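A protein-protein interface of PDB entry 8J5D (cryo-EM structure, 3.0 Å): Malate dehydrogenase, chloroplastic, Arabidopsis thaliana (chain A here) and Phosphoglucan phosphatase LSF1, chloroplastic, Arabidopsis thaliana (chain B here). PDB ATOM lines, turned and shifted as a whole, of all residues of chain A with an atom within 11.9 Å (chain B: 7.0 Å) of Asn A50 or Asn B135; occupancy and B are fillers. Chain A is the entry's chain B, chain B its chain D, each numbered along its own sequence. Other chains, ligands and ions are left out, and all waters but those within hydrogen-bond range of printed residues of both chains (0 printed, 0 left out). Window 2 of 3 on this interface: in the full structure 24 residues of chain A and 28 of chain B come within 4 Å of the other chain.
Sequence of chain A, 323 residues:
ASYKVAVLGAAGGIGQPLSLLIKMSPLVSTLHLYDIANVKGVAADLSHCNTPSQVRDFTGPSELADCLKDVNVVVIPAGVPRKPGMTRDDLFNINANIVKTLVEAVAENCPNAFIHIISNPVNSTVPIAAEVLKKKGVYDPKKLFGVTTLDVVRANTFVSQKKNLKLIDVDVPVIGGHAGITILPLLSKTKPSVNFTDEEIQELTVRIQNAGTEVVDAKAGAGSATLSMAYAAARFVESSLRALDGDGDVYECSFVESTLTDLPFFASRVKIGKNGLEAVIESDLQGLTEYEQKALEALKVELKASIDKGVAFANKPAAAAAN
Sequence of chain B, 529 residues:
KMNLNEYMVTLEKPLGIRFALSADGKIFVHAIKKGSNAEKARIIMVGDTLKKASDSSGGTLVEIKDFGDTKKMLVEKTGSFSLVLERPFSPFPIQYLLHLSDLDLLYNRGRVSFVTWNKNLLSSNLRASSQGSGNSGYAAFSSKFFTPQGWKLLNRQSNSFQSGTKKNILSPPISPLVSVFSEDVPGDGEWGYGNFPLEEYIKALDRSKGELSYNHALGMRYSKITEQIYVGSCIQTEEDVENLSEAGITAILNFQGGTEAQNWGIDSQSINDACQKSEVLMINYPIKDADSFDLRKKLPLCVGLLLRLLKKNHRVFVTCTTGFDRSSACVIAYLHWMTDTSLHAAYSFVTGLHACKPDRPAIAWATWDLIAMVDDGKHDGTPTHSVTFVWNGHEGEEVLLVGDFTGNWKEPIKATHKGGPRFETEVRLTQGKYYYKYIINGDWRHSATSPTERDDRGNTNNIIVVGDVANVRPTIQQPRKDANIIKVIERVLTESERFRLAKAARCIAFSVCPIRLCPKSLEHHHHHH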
ATOM      1  N   SER A  19      21.124  23.396 -12.104  1.00  0.00           N
ATOM      2  CA  SER A  19      20.211  24.217 -12.886  1.00  0.00           C
ATOM      3  C   SER A  19      20.422  23.998 -14.375  1.00  0.00           C
ATOM      4  O   SER A  19      19.454  23.902 -15.139  1.00  0.00           O
ATOM      5  CB  SER A  19      20.397  25.689 -12.524  1.00  0.00           C
ATOM      6  OG  SER A  19      20.078  25.920 -11.165  1.00  0.00           O
ATOM      7  N   LEU A  20      21.684  23.905 -14.805  1.00  0.00           N
ATOM      8  CA  LEU A  20      21.959  23.616 -16.210  1.00  0.00           C
ATOM      9  C   LEU A  20      21.341  22.288 -16.629  1.00  0.00           C
ATOM     10  O   LEU A  20      20.677  22.201 -17.672  1.00  0.00           O
ATOM     11  CB  LEU A  20      23.466  23.602 -16.460  1.00  0.00           C
ATOM     12  CG  LEU A  20      23.919  23.104 -17.835  1.00  0.00           C
ATOM     13  CD1 LEU A  20      23.476  24.059 -18.926  1.00  0.00           C
ATOM     14  CD2 LEU A  20      25.423  22.894 -17.875  1.00  0.00           C
ATOM     15  N   LEU A  21      21.531  21.245 -15.820  1.00  0.00           N
ATOM     16  CA  LEU A  21      21.019  19.929 -16.179  1.00  0.00           C
ATOM     17  C   LEU A  21      19.500  19.887 -16.174  1.00  0.00           C
ATOM     18  O   LEU A  21      18.901  19.204 -17.011  1.00  0.00           O
ATOM     19  CB  LEU A  21      21.573  18.870 -15.230  1.00  0.00           C
ATOM     20  CG  LEU A  21      23.043  18.545 -15.462  1.00  0.00           C
ATOM     21  CD1 LEU A  21      23.389  17.178 -14.900  1.00  0.00           C
ATOM     22  CD2 LEU A  21      23.370  18.642 -16.938  1.00  0.00           C
ATOM     23  N   ILE A  22      18.857  20.587 -15.239  1.00  0.00           N
ATOM     24  CA  ILE A  22      17.401  20.553 -15.195  1.00  0.00           C
ATOM     25  C   ILE A  22      16.820  21.366 -16.345  1.00  0.00           C
ATOM     26  O   ILE A  22      15.768  21.020 -16.896  1.00  0.00           O
ATOM     27  CB  ILE A  22      16.883  21.035 -13.829  1.00  0.00           C
ATOM     28  CG1 ILE A  22      17.327  20.084 -12.724  1.00  0.00           C
ATOM     29  CG2 ILE A  22      15.381  20.994 -13.808  1.00  0.00           C
ATOM     30  CD1 ILE A  22      17.000  20.591 -11.340  1.00  0.00           C
ATOM     31  N   LYS A  23      17.493  22.454 -16.734  1.00  0.00           N
ATOM     32  CA  LYS A  23      17.058  23.193 -17.916  1.00  0.00           C
ATOM     33  C   LYS A  23      17.193  22.348 -19.174  1.00  0.00           C
ATOM     34  O   LYS A  23      16.313  22.364 -20.040  1.00  0.00           O
ATOM     35  CB  LYS A  23      17.850  24.489 -18.066  1.00  0.00           C
ATOM     36  CG  LYS A  23      17.368  25.335 -19.228  1.00  0.00           C
ATOM     37  CD  LYS A  23      18.084  26.662 -19.304  1.00  0.00           C
ATOM     38  CE  LYS A  23      17.716  27.395 -20.580  1.00  0.00           C
ATOM     39  NZ  LYS A  23      16.302  27.847 -20.585  1.00  0.00           N
ATOM     40  N   MET A  24      18.286  21.595 -19.291  1.00  0.00           N
ATOM     41  CA  MET A  24      18.466  20.743 -20.459  1.00  0.00           C
ATOM     42  C   MET A  24      17.684  19.445 -20.310  1.00  0.00           C
ATOM     43  O   MET A  24      18.248  18.356 -20.453  1.00  0.00           O
ATOM     44  CB  MET A  24      19.946  20.440 -20.680  1.00  0.00           C
ATOM     45  CG  MET A  24      20.775  21.648 -21.058  1.00  0.00           C
ATOM     46  SD  MET A  24      22.530  21.287 -20.936  1.00  0.00           S
ATOM     47  CE  MET A  24      22.566  19.656 -21.659  1.00  0.00           C
ATOM     48  N   SER A  25      16.386  19.550 -20.034  1.00  0.00           N
ATOM     49  CA  SER A  25      15.541  18.384 -19.841  1.00  0.00           C
ATOM     50  C   SER A  25      14.275  18.516 -20.674  1.00  0.00           C
ATOM     51  O   SER A  25      13.772  19.628 -20.875  1.00  0.00           O
ATOM     52  CB  SER A  25      15.173  18.212 -18.364  1.00  0.00           C
ATOM     53  OG  SER A  25      14.056  19.015 -18.033  1.00  0.00           O
ATOM     54  N   PRO A  26      13.732  17.399 -21.168  1.00  0.00           N
ATOM     55  CA  PRO A  26      12.532  17.469 -22.012  1.00  0.00           C
ATOM     56  C   PRO A  26      11.240  17.687 -21.246  1.00  0.00           C
ATOM     57  O   PRO A  26      10.221  18.009 -21.870  1.00  0.00           O
ATOM     58  CB  PRO A  26      12.525  16.106 -22.714  1.00  0.00           C
ATOM     59  CG  PRO A  26      13.232  15.202 -21.771  1.00  0.00           C
ATOM     60  CD  PRO A  26      14.264  16.028 -21.066  1.00  0.00           C
ATOM     61  N   VAL A  28      10.880  19.662 -18.096  1.00  0.00           N
ATOM     62  CA  VAL A  28      10.735  20.964 -17.458  1.00  0.00           C
ATOM     63  C   VAL A  28      10.352  22.003 -18.499  1.00  0.00           C
ATOM     64  O   VAL A  28      10.986  22.113 -19.556  1.00  0.00           O
ATOM     65  CB  VAL A  28      12.031  21.360 -16.737  1.00  0.00           C
ATOM     66  CG1 VAL A  28      11.883  22.731 -16.099  1.00  0.00           C
ATOM     67  CG2 VAL A  28      12.389  20.328 -15.695  1.00  0.00           C
ATOM     68  N   SER A  29       9.302  22.771 -18.207  1.00  0.00           N
ATOM     69  CA  SER A  29       8.945  23.920 -19.022  1.00  0.00           C
ATOM     70  C   SER A  29       9.278  25.244 -18.355  1.00  0.00           C
ATOM     71  O   SER A  29       9.560  26.219 -19.059  1.00  0.00           O
ATOM     72  CB  SER A  29       7.448  23.898 -19.360  1.00  0.00           C
ATOM     73  OG  SER A  29       6.661  23.902 -18.184  1.00  0.00           O
ATOM     74  N   VAL A  42      23.635  33.540 -12.881  1.00  0.00           N
ATOM     75  CA  VAL A  42      23.408  32.178 -13.353  1.00  0.00           C
ATOM     76  C   VAL A  42      22.159  32.113 -14.224  1.00  0.00           C
ATOM     77  O   VAL A  42      22.124  31.395 -15.231  1.00  0.00           O
ATOM     78  CB  VAL A  42      23.324  31.208 -12.159  1.00  0.00           C
ATOM     79  CG1 VAL A  42      22.965  29.807 -12.629  1.00  0.00           C
ATOM     80  CG2 VAL A  42      24.638  31.198 -11.397  1.00  0.00           C
ATOM     81  N   ALA A  43      21.116  32.861 -13.859  1.00  0.00           N
ATOM     82  CA  ALA A  43      19.902  32.877 -14.669  1.00  0.00           C
ATOM     83  C   ALA A  43      20.160  33.478 -16.043  1.00  0.00           C
ATOM     84  O   ALA A  43      19.675  32.958 -17.055  1.00  0.00           O
ATOM     85  CB  ALA A  43      18.798  33.646 -13.950  1.00  0.00           C
ATOM     86  N   ALA A  44      20.915  34.579 -16.102  1.00  0.00           N
ATOM     87  CA  ALA A  44      21.258  35.172 -17.390  1.00  0.00           C
ATOM     88  C   ALA A  44      22.139  34.237 -18.205  1.00  0.00           C
ATOM     89  O   ALA A  44      21.991  34.139 -19.428  1.00  0.00           O
ATOM     90  CB  ALA A  44      21.948  36.518 -17.181  1.00  0.00           C
ATOM     91  N   ASP A  45      23.066  33.543 -17.543  1.00  0.00           N
ATOM     92  CA  ASP A  45      23.905  32.572 -18.234  1.00  0.00           C
ATOM     93  C   ASP A  45      23.066  31.457 -18.843  1.00  0.00           C
ATOM     94  O   ASP A  45      23.299  31.047 -19.985  1.00  0.00           O
ATOM     95  CB  ASP A  45      24.936  32.002 -17.260  1.00  0.00           C
ATOM     96  CG  ASP A  45      25.992  31.166 -17.948  1.00  0.00           C
ATOM     97  OD1 ASP A  45      26.036  31.166 -19.193  1.00  0.00           O
ATOM     98  OD2 ASP A  45      26.779  30.504 -17.240  1.00  0.00           O
ATOM     99  N   LEU A  46      22.079  30.958 -18.099  1.00  0.00           N
ATOM    100  CA  LEU A  46      21.276  29.843 -18.587  1.00  0.00           C
ATOM    101  C   LEU A  46      20.264  30.268 -19.639  1.00  0.00           C
ATOM    102  O   LEU A  46      19.967  29.489 -20.549  1.00  0.00           O
ATOM    103  CB  LEU A  46      20.552  29.162 -17.428  1.00  0.00           C
ATOM    104  CG  LEU A  46      21.351  28.107 -16.670  1.00  0.00           C
ATOM    105  CD1 LEU A  46      20.485  27.485 -15.598  1.00  0.00           C
ATOM    106  CD2 LEU A  46      21.877  27.053 -17.625  1.00  0.00           C
ATOM    107  N   SER A  47      19.736  31.490 -19.548  1.00  0.00           N
ATOM    108  CA  SER A  47      18.700  31.925 -20.477  1.00  0.00           C
ATOM    109  C   SER A  47      19.185  31.983 -21.918  1.00  0.00           C
ATOM    110  O   SER A  47      18.353  32.048 -22.828  1.00  0.00           O
ATOM    111  CB  SER A  47      18.168  33.296 -20.061  1.00  0.00           C
ATOM    112  OG  SER A  47      19.103  34.314 -20.368  1.00  0.00           O
ATOM    113  N   HIS A  48      20.497  31.963 -22.146  1.00  0.00           N
ATOM    114  CA  HIS A  48      21.039  32.005 -23.496  1.00  0.00           C
ATOM    115  C   HIS A  48      21.053  30.645 -24.180  1.00  0.00           C
ATOM    116  O   HIS A  48      21.223  30.592 -25.401  1.00  0.00           O
ATOM    117  CB  HIS A  48      22.450  32.591 -23.465  1.00  0.00           C
ATOM    118  CG  HIS A  48      22.489  34.029 -23.060  1.00  0.00           C
ATOM    119  ND1 HIS A  48      23.667  34.719 -22.866  1.00  0.00           N
ATOM    120  CD2 HIS A  48      21.492  34.911 -22.813  1.00  0.00           C
ATOM    121  CE1 HIS A  48      23.392  35.963 -22.518  1.00  0.00           C
ATOM    122  NE2 HIS A  48      22.079  36.105 -22.478  1.00  0.00           N
ATOM    123  N   CYS A  49      20.880  29.555 -23.438  1.00  0.00           N
ATOM    124  CA  CYS A  49      20.754  28.248 -24.065  1.00  0.00           C
ATOM    125  C   CYS A  49      19.420  28.145 -24.798  1.00  0.00           C
ATOM    126  O   CYS A  49      18.408  28.710 -24.376  1.00  0.00           O
ATOM    127  CB  CYS A  49      20.869  27.140 -23.019  1.00  0.00           C
ATOM    128  SG  CYS A  49      22.453  27.099 -22.156  1.00  0.00           S
ATOM    129  N   ASN A  50      19.427  27.420 -25.912  1.00  0.00           N
ATOM    130  CA  ASN A  50      18.251  27.343 -26.778  1.00  0.00           C
ATOM    131  C   ASN A  50      17.352  26.161 -26.428  1.00  0.00           C
ATOM    132  O   ASN A  50      16.940  25.395 -27.294  1.00  0.00           O
ATOM    133  CB  ASN A  50      18.691  27.284 -28.236  1.00  0.00           C
ATOM    134  CG  ASN A  50      19.628  26.127 -28.516  1.00  0.00           C
ATOM    135  OD1 ASN A  50      20.190  25.531 -27.597  1.00  0.00           O
ATOM    136  ND2 ASN A  50      19.805  25.803 -29.791  1.00  0.00           N
ATOM    137  N   THR A  51      17.008  26.025 -25.149  1.00  0.00           N
ATOM    138  CA  THR A  51      16.102  24.966 -24.736  1.00  0.00           C
ATOM    139  C   THR A  51      14.754  25.551 -24.331  1.00  0.00           C
ATOM    140  O   THR A  51      14.687  26.677 -23.826  1.00  0.00           O
ATOM    141  CB  THR A  51      16.677  24.156 -23.568  1.00  0.00           C
ATOM    142  OG1 THR A  51      17.299  25.041 -22.630  1.00  0.00           O
ATOM    143  CG2 THR A  51      17.699  23.147 -24.068  1.00  0.00           C
ATOM    144  N   PRO A  52      13.659  24.814 -24.543  1.00  0.00           N
ATOM    145  CA  PRO A  52      12.327  25.391 -24.292  1.00  0.00           C
ATOM    146  C   PRO A  52      12.103  25.830 -22.855  1.00  0.00           C
ATOM    147  O   PRO A  52      11.303  26.745 -22.620  1.00  0.00           O
ATOM    148  CB  PRO A  52      11.376  24.253 -24.686  1.00  0.00           C
ATOM    149  CG  PRO A  52      12.169  23.394 -25.608  1.00  0.00           C
ATOM    150  CD  PRO A  52      13.572  23.455 -25.102  1.00  0.00           C
ATOM    151  N   SER A  53      12.774  25.203 -21.890  1.00  0.00           N
ATOM    152  CA  SER A  53      12.579  25.524 -20.482  1.00  0.00           C
ATOM    153  C   SER A  53      12.909  26.981 -20.193  1.00  0.00           C
ATOM    154  O   SER A  53      14.071  27.388 -20.281  1.00  0.00           O
ATOM    155  CB  SER A  53      13.439  24.611 -19.606  1.00  0.00           C
ATOM    156  OG  SER A  53      13.441  23.286 -20.104  1.00  0.00           O
ATOM    157  N   GLN A  54      11.899  27.774 -19.847  1.00  0.00           N
ATOM    158  CA  GLN A  54      12.144  29.151 -19.449  1.00  0.00           C
ATOM    159  C   GLN A  54      12.867  29.181 -18.110  1.00  0.00           C
ATOM    160  O   GLN A  54      12.797  28.233 -17.328  1.00  0.00           O
ATOM    161  CB  GLN A  54      10.831  29.926 -19.355  1.00  0.00           C
ATOM    162  CG  GLN A  54      10.046  29.970 -20.651  1.00  0.00           C
ATOM    163  CD  GLN A  54      10.814  30.640 -21.771  1.00  0.00           C
ATOM    164  OE1 GLN A  54      11.071  31.843 -21.730  1.00  0.00           O
ATOM    165  NE2 GLN A  54      11.188  29.861 -22.779  1.00  0.00           N
ATOM    166  N   VAL A  55      13.576  30.276 -17.852  1.00  0.00           N
ATOM    167  CA  VAL A  55      14.348  30.436 -16.625  1.00  0.00           C
ATOM    168  C   VAL A  55      14.004  31.779 -16.000  1.00  0.00           C
ATOM    169  O   VAL A  55      14.038  32.813 -16.677  1.00  0.00           O
ATOM    170  CB  VAL A  55      15.863  30.331 -16.886  1.00  0.00           C
ATOM    171  CG1 VAL A  55      16.647  30.968 -15.754  1.00  0.00           C
ATOM    172  CG2 VAL A  55      16.265  28.878 -17.052  1.00  0.00           C
ATOM    173  N   TRP B 117      22.347  16.406 -29.089  1.00  0.00           N
ATOM    174  CA  TRP B 117      21.811  17.441 -29.954  1.00  0.00           C
ATOM    175  C   TRP B 117      21.361  16.898 -31.300  1.00  0.00           C
ATOM    176  O   TRP B 117      20.759  17.644 -32.079  1.00  0.00           O
ATOM    177  CB  TRP B 117      22.855  18.545 -30.186  1.00  0.00           C
ATOM    178  CG  TRP B 117      23.124  19.398 -28.986  1.00  0.00           C
ATOM    179  CD1 TRP B 117      22.694  20.673 -28.778  1.00  0.00           C
ATOM    180  CD2 TRP B 117      23.889  19.041 -27.827  1.00  0.00           C
ATOM    181  NE1 TRP B 117      23.138  21.132 -27.564  1.00  0.00           N
ATOM    182  CE2 TRP B 117      23.875  20.148 -26.961  1.00  0.00           C
ATOM    183  CE3 TRP B 117      24.584  17.892 -27.440  1.00  0.00           C
ATOM    184  CZ2 TRP B 117      24.527  20.140 -25.732  1.00  0.00           C
ATOM    185  CZ3 TRP B 117      25.230  17.888 -26.222  1.00  0.00           C
ATOM    186  CH2 TRP B 117      25.197  19.004 -25.382  1.00  0.00           C
ATOM    187  N   ASN B 118      21.627  15.627 -31.587  1.00  0.00           N
ATOM    188  CA  ASN B 118      21.272  15.019 -32.860  1.00  0.00           C
ATOM    189  C   ASN B 118      19.790  14.673 -32.860  1.00  0.00           C
ATOM    190  O   ASN B 118      19.352  13.810 -32.092  1.00  0.00           O
ATOM    191  CB  ASN B 118      22.121  13.771 -33.093  1.00  0.00           C
ATOM    192  CG  ASN B 118      21.948  13.194 -34.483  1.00  0.00           C
ATOM    193  OD1 ASN B 118      21.185  13.714 -35.295  1.00  0.00           O
ATOM    194  ND2 ASN B 118      22.661  12.110 -34.763  1.00  0.00           N
ATOM    195  N   LYS B 119      19.019  15.343 -33.720  1.00  0.00           N
ATOM    196  CA  LYS B 119      17.583  15.105 -33.769  1.00  0.00           C
ATOM    197  C   LYS B 119      17.245  13.685 -34.199  1.00  0.00           C
ATOM    198  O   LYS B 119      16.165  13.192 -33.865  1.00  0.00           O
ATOM    199  CB  LYS B 119      16.910  16.112 -34.705  1.00  0.00           C
ATOM    200  CG  LYS B 119      16.679  15.603 -36.118  1.00  0.00           C
ATOM    201  CD  LYS B 119      16.006  16.652 -36.984  1.00  0.00           C
ATOM    202  CE  LYS B 119      16.113  16.295 -38.455  1.00  0.00           C
ATOM    203  NZ  LYS B 119      15.608  17.388 -39.330  1.00  0.00           N
ATOM    204  N   ARG B 127      12.178  16.600 -32.048  1.00  0.00           N
ATOM    205  CA  ARG B 127      12.963  16.606 -33.279  1.00  0.00           C
ATOM    206  C   ARG B 127      12.900  17.964 -33.969  1.00  0.00           C
ATOM    207  O   ARG B 127      13.934  18.580 -34.254  1.00  0.00           O
ATOM    208  CB  ARG B 127      12.454  15.514 -34.220  1.00  0.00           C
ATOM    209  CG  ARG B 127      13.277  14.247 -34.238  1.00  0.00           C
ATOM    210  CD  ARG B 127      12.542  13.147 -34.985  1.00  0.00           C
ATOM    211  NE  ARG B 127      13.434  12.075 -35.411  1.00  0.00           N
ATOM    212  CZ  ARG B 127      13.368  10.828 -34.967  1.00  0.00           C
ATOM    213  NH1 ARG B 127      12.460  10.458 -34.080  1.00  0.00           N
ATOM    214  NH2 ARG B 127      14.232   9.928 -35.429  1.00  0.00           N
ATOM    215  N   ALA B 128      11.682  18.415 -34.285  1.00  0.00           N
ATOM    216  CA  ALA B 128      11.357  19.638 -35.017  1.00  0.00           C
ATOM    217  C   ALA B 128      11.694  19.517 -36.500  1.00  0.00           C
ATOM    218  O   ALA B 128      11.295  20.375 -37.292  1.00  0.00           O
ATOM    219  CB  ALA B 128      12.063  20.856 -34.410  1.00  0.00           C
ATOM    220  N   SER B 130      13.361  19.950 -39.263  1.00  0.00           N
ATOM    221  CA  SER B 130      13.275  21.094 -40.160  1.00  0.00           C
ATOM    222  C   SER B 130      14.358  21.108 -41.232  1.00  0.00           C
ATOM    223  O   SER B 130      14.042  21.025 -42.422  1.00  0.00           O
ATOM    224  CB  SER B 130      13.335  22.388 -39.339  1.00  0.00           C
ATOM    225  OG  SER B 130      13.090  23.526 -40.149  1.00  0.00           O
ATOM    226  N   GLN B 131      15.631  21.207 -40.855  1.00  0.00           N
ATOM    227  CA  GLN B 131      16.702  21.239 -41.844  1.00  0.00           C
ATOM    228  C   GLN B 131      17.776  20.190 -41.606  1.00  0.00           C
ATOM    229  O   GLN B 131      18.138  19.458 -42.536  1.00  0.00           O
ATOM    230  CB  GLN B 131      17.333  22.638 -41.888  1.00  0.00           C
ATOM    231  CG  GLN B 131      16.381  23.719 -42.377  1.00  0.00           C
ATOM    232  CD  GLN B 131      15.837  23.435 -43.763  1.00  0.00           C
ATOM    233  OE1 GLN B 131      16.593  23.164 -44.696  1.00  0.00           O
ATOM    234  NE2 GLN B 131      14.518  23.495 -43.905  1.00  0.00           N
ATOM    235  N   GLY B 132      18.298  20.096 -40.386  1.00  0.00           N
ATOM    236  CA  GLY B 132      19.435  19.241 -40.114  1.00  0.00           C
ATOM    237  C   GLY B 132      19.380  18.576 -38.755  1.00  0.00           C
ATOM    238  O   GLY B 132      18.321  18.529 -38.125  1.00  0.00           O
ATOM    239  N   SER B 133      20.523  18.079 -38.284  1.00  0.00           N
ATOM    240  CA  SER B 133      20.561  17.265 -37.074  1.00  0.00           C
ATOM    241  C   SER B 133      20.385  18.094 -35.808  1.00  0.00           C
ATOM    242  O   SER B 133      21.313  18.212 -35.001  1.00  0.00           O
ATOM    243  CB  SER B 133      21.874  16.484 -37.008  1.00  0.00           C
ATOM    244  OG  SER B 133      21.947  15.529 -38.051  1.00  0.00           O
ATOM    245  N   GLY B 134      19.205  18.670 -35.626  1.00  0.00           N
ATOM    246  CA  GLY B 134      18.826  19.265 -34.363  1.00  0.00           C
ATOM    247  C   GLY B 134      19.477  20.612 -34.106  1.00  0.00           C
ATOM    248  O   GLY B 134      20.520  20.959 -34.658  1.00  0.00           O
ATOM    249  N   ASN B 135      18.831  21.381 -33.238  1.00  0.00           N
ATOM    250  CA  ASN B 135      19.323  22.676 -32.787  1.00  0.00           C
ATOM    251  C   ASN B 135      19.584  22.720 -31.293  1.00  0.00           C
ATOM    252  O   ASN B 135      20.591  23.288 -30.863  1.00  0.00           O
ATOM    253  CB  ASN B 135      18.322  23.780 -33.152  1.00  0.00           C
ATOM    254  CG  ASN B 135      18.173  23.959 -34.644  1.00  0.00           C
ATOM    255  OD1 ASN B 135      19.118  23.753 -35.402  1.00  0.00           O
ATOM    256  ND2 ASN B 135      16.978  24.341 -35.075  1.00  0.00           N
ATOM    257  N   SER B 136      18.700  22.138 -30.490  1.00  0.00           N
ATOM    258  CA  SER B 136      18.832  22.114 -29.043  1.00  0.00           C
ATOM    259  C   SER B 136      19.138  20.701 -28.568  1.00  0.00           C
ATOM    260  O   SER B 136      18.743  19.711 -29.187  1.00  0.00           O
ATOM    261  CB  SER B 136      17.557  22.622 -28.367  1.00  0.00           C
ATOM    262  OG  SER B 136      16.493  21.708 -28.536  1.00  0.00           O
ATOM    263  N   GLY B 137      19.849  20.623 -27.449  1.00  0.00           N
ATOM    264  CA  GLY B 137      20.246  19.355 -26.875  1.00  0.00           C
ATOM    265  C   GLY B 137      19.522  19.099 -25.570  1.00  0.00           C
ATOM    266  O   GLY B 137      19.222  20.024 -24.815  1.00  0.00           O
ATOM    267  N   TYR B 138      19.241  17.828 -25.314  1.00  0.00           N
ATOM    268  CA  TYR B 138      18.538  17.400 -24.119  1.00  0.00           C
ATOM    269  C   TYR B 138      19.405  16.430 -23.332  1.00  0.00           C
ATOM    270  O   TYR B 138      20.137  15.614 -23.907  1.00  0.00           O
ATOM    271  CB  TYR B 138      17.201  16.737 -24.466  1.00  0.00           C
ATOM    272  CG  TYR B 138      16.197  17.681 -25.080  1.00  0.00           C
ATOM    273  CD1 TYR B 138      15.556  18.637 -24.307  1.00  0.00           C
ATOM    274  CD2 TYR B 138      15.890  17.616 -26.430  1.00  0.00           C
ATOM    275  CE1 TYR B 138      14.637  19.501 -24.860  1.00  0.00           C
ATOM    276  CE2 TYR B 138      14.973  18.478 -26.994  1.00  0.00           C
ATOM    277  CZ  TYR B 138      14.349  19.418 -26.204  1.00  0.00           C
ATOM    278  OH  TYR B 138      13.433  20.280 -26.757  1.00  0.00           O
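The backbone carbonyl oxygen of Asn B135 is in hydrogen-bond range of the side-chain amide nitrogen of Asn A50 (2.8 Å).
O of Met A24 touches C of Tyr B138, 3.7 Å away.
Tyr B138 touches Ser A25.
N of Pro A26 touches CD1 of Tyr B138, 3.8 Å away.
Ser B136 touches Asn A50.
CG2 of Thr A51 touches O of Gly B137 (3.6 Å).
Tyr B138 touches Pro A52.
Printed residues of chain B within 4 Å of Pro A26: Tyr B138.
Asn A50 touches just these residues of chain B: Asn B135 (2.8 Å) and Ser B136 (3.0 Å).
Printed residues of chain B within 4 Å of Thr A51: Gly B137 (3.6 Å).
Printed residues of chain B within 4 Å of Pro A52: Tyr B138 (3.6 Å).
No residue of chain A comes within 4 Å of Ala B128.
Gly B132 touches none of the printed residues of chain A.
No residue of chain A comes within 4 Å of Gly B134.
Asn B135 touches one residue of chain A.
Ser B136 touches just one residue of chain A: Asn A50 (3.0 Å).
Gly B137 touches just one residue of chain A: Thr A51 (3.6 Å).
Printed residues of chain A within 4 Å of Tyr B138: Met A24, Ser A25, Pro A26 and Pro A52.
The nearest residue of chain A that does not touch Asn B135 is Thr A51 (7.3 Å).
The backbone NH (N) of Val A28 sits close to the side-chain hydroxyl (OG) of Ser A25.
The side-chain amide nitrogen of Gln A54 is in hydrogen-bond range of the backbone carbonyl oxygen of Pro A52.
The backbone carbonyl oxygen (O) of Ile A22 sits at hydrogen-bond distance from the side-chain hydroxyl (OG) of Ser A25, at 2.9 Å.
Of the 14 printed residues of chain B, 4 touch a printed residue of chain A.
Among the printed residues, 7 pairs touch across the chains.
Among the printed residues, no Asp or Glu carboxylate lies within 4 Å of a Lys or Arg side-chain nitrogen of the other chain.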
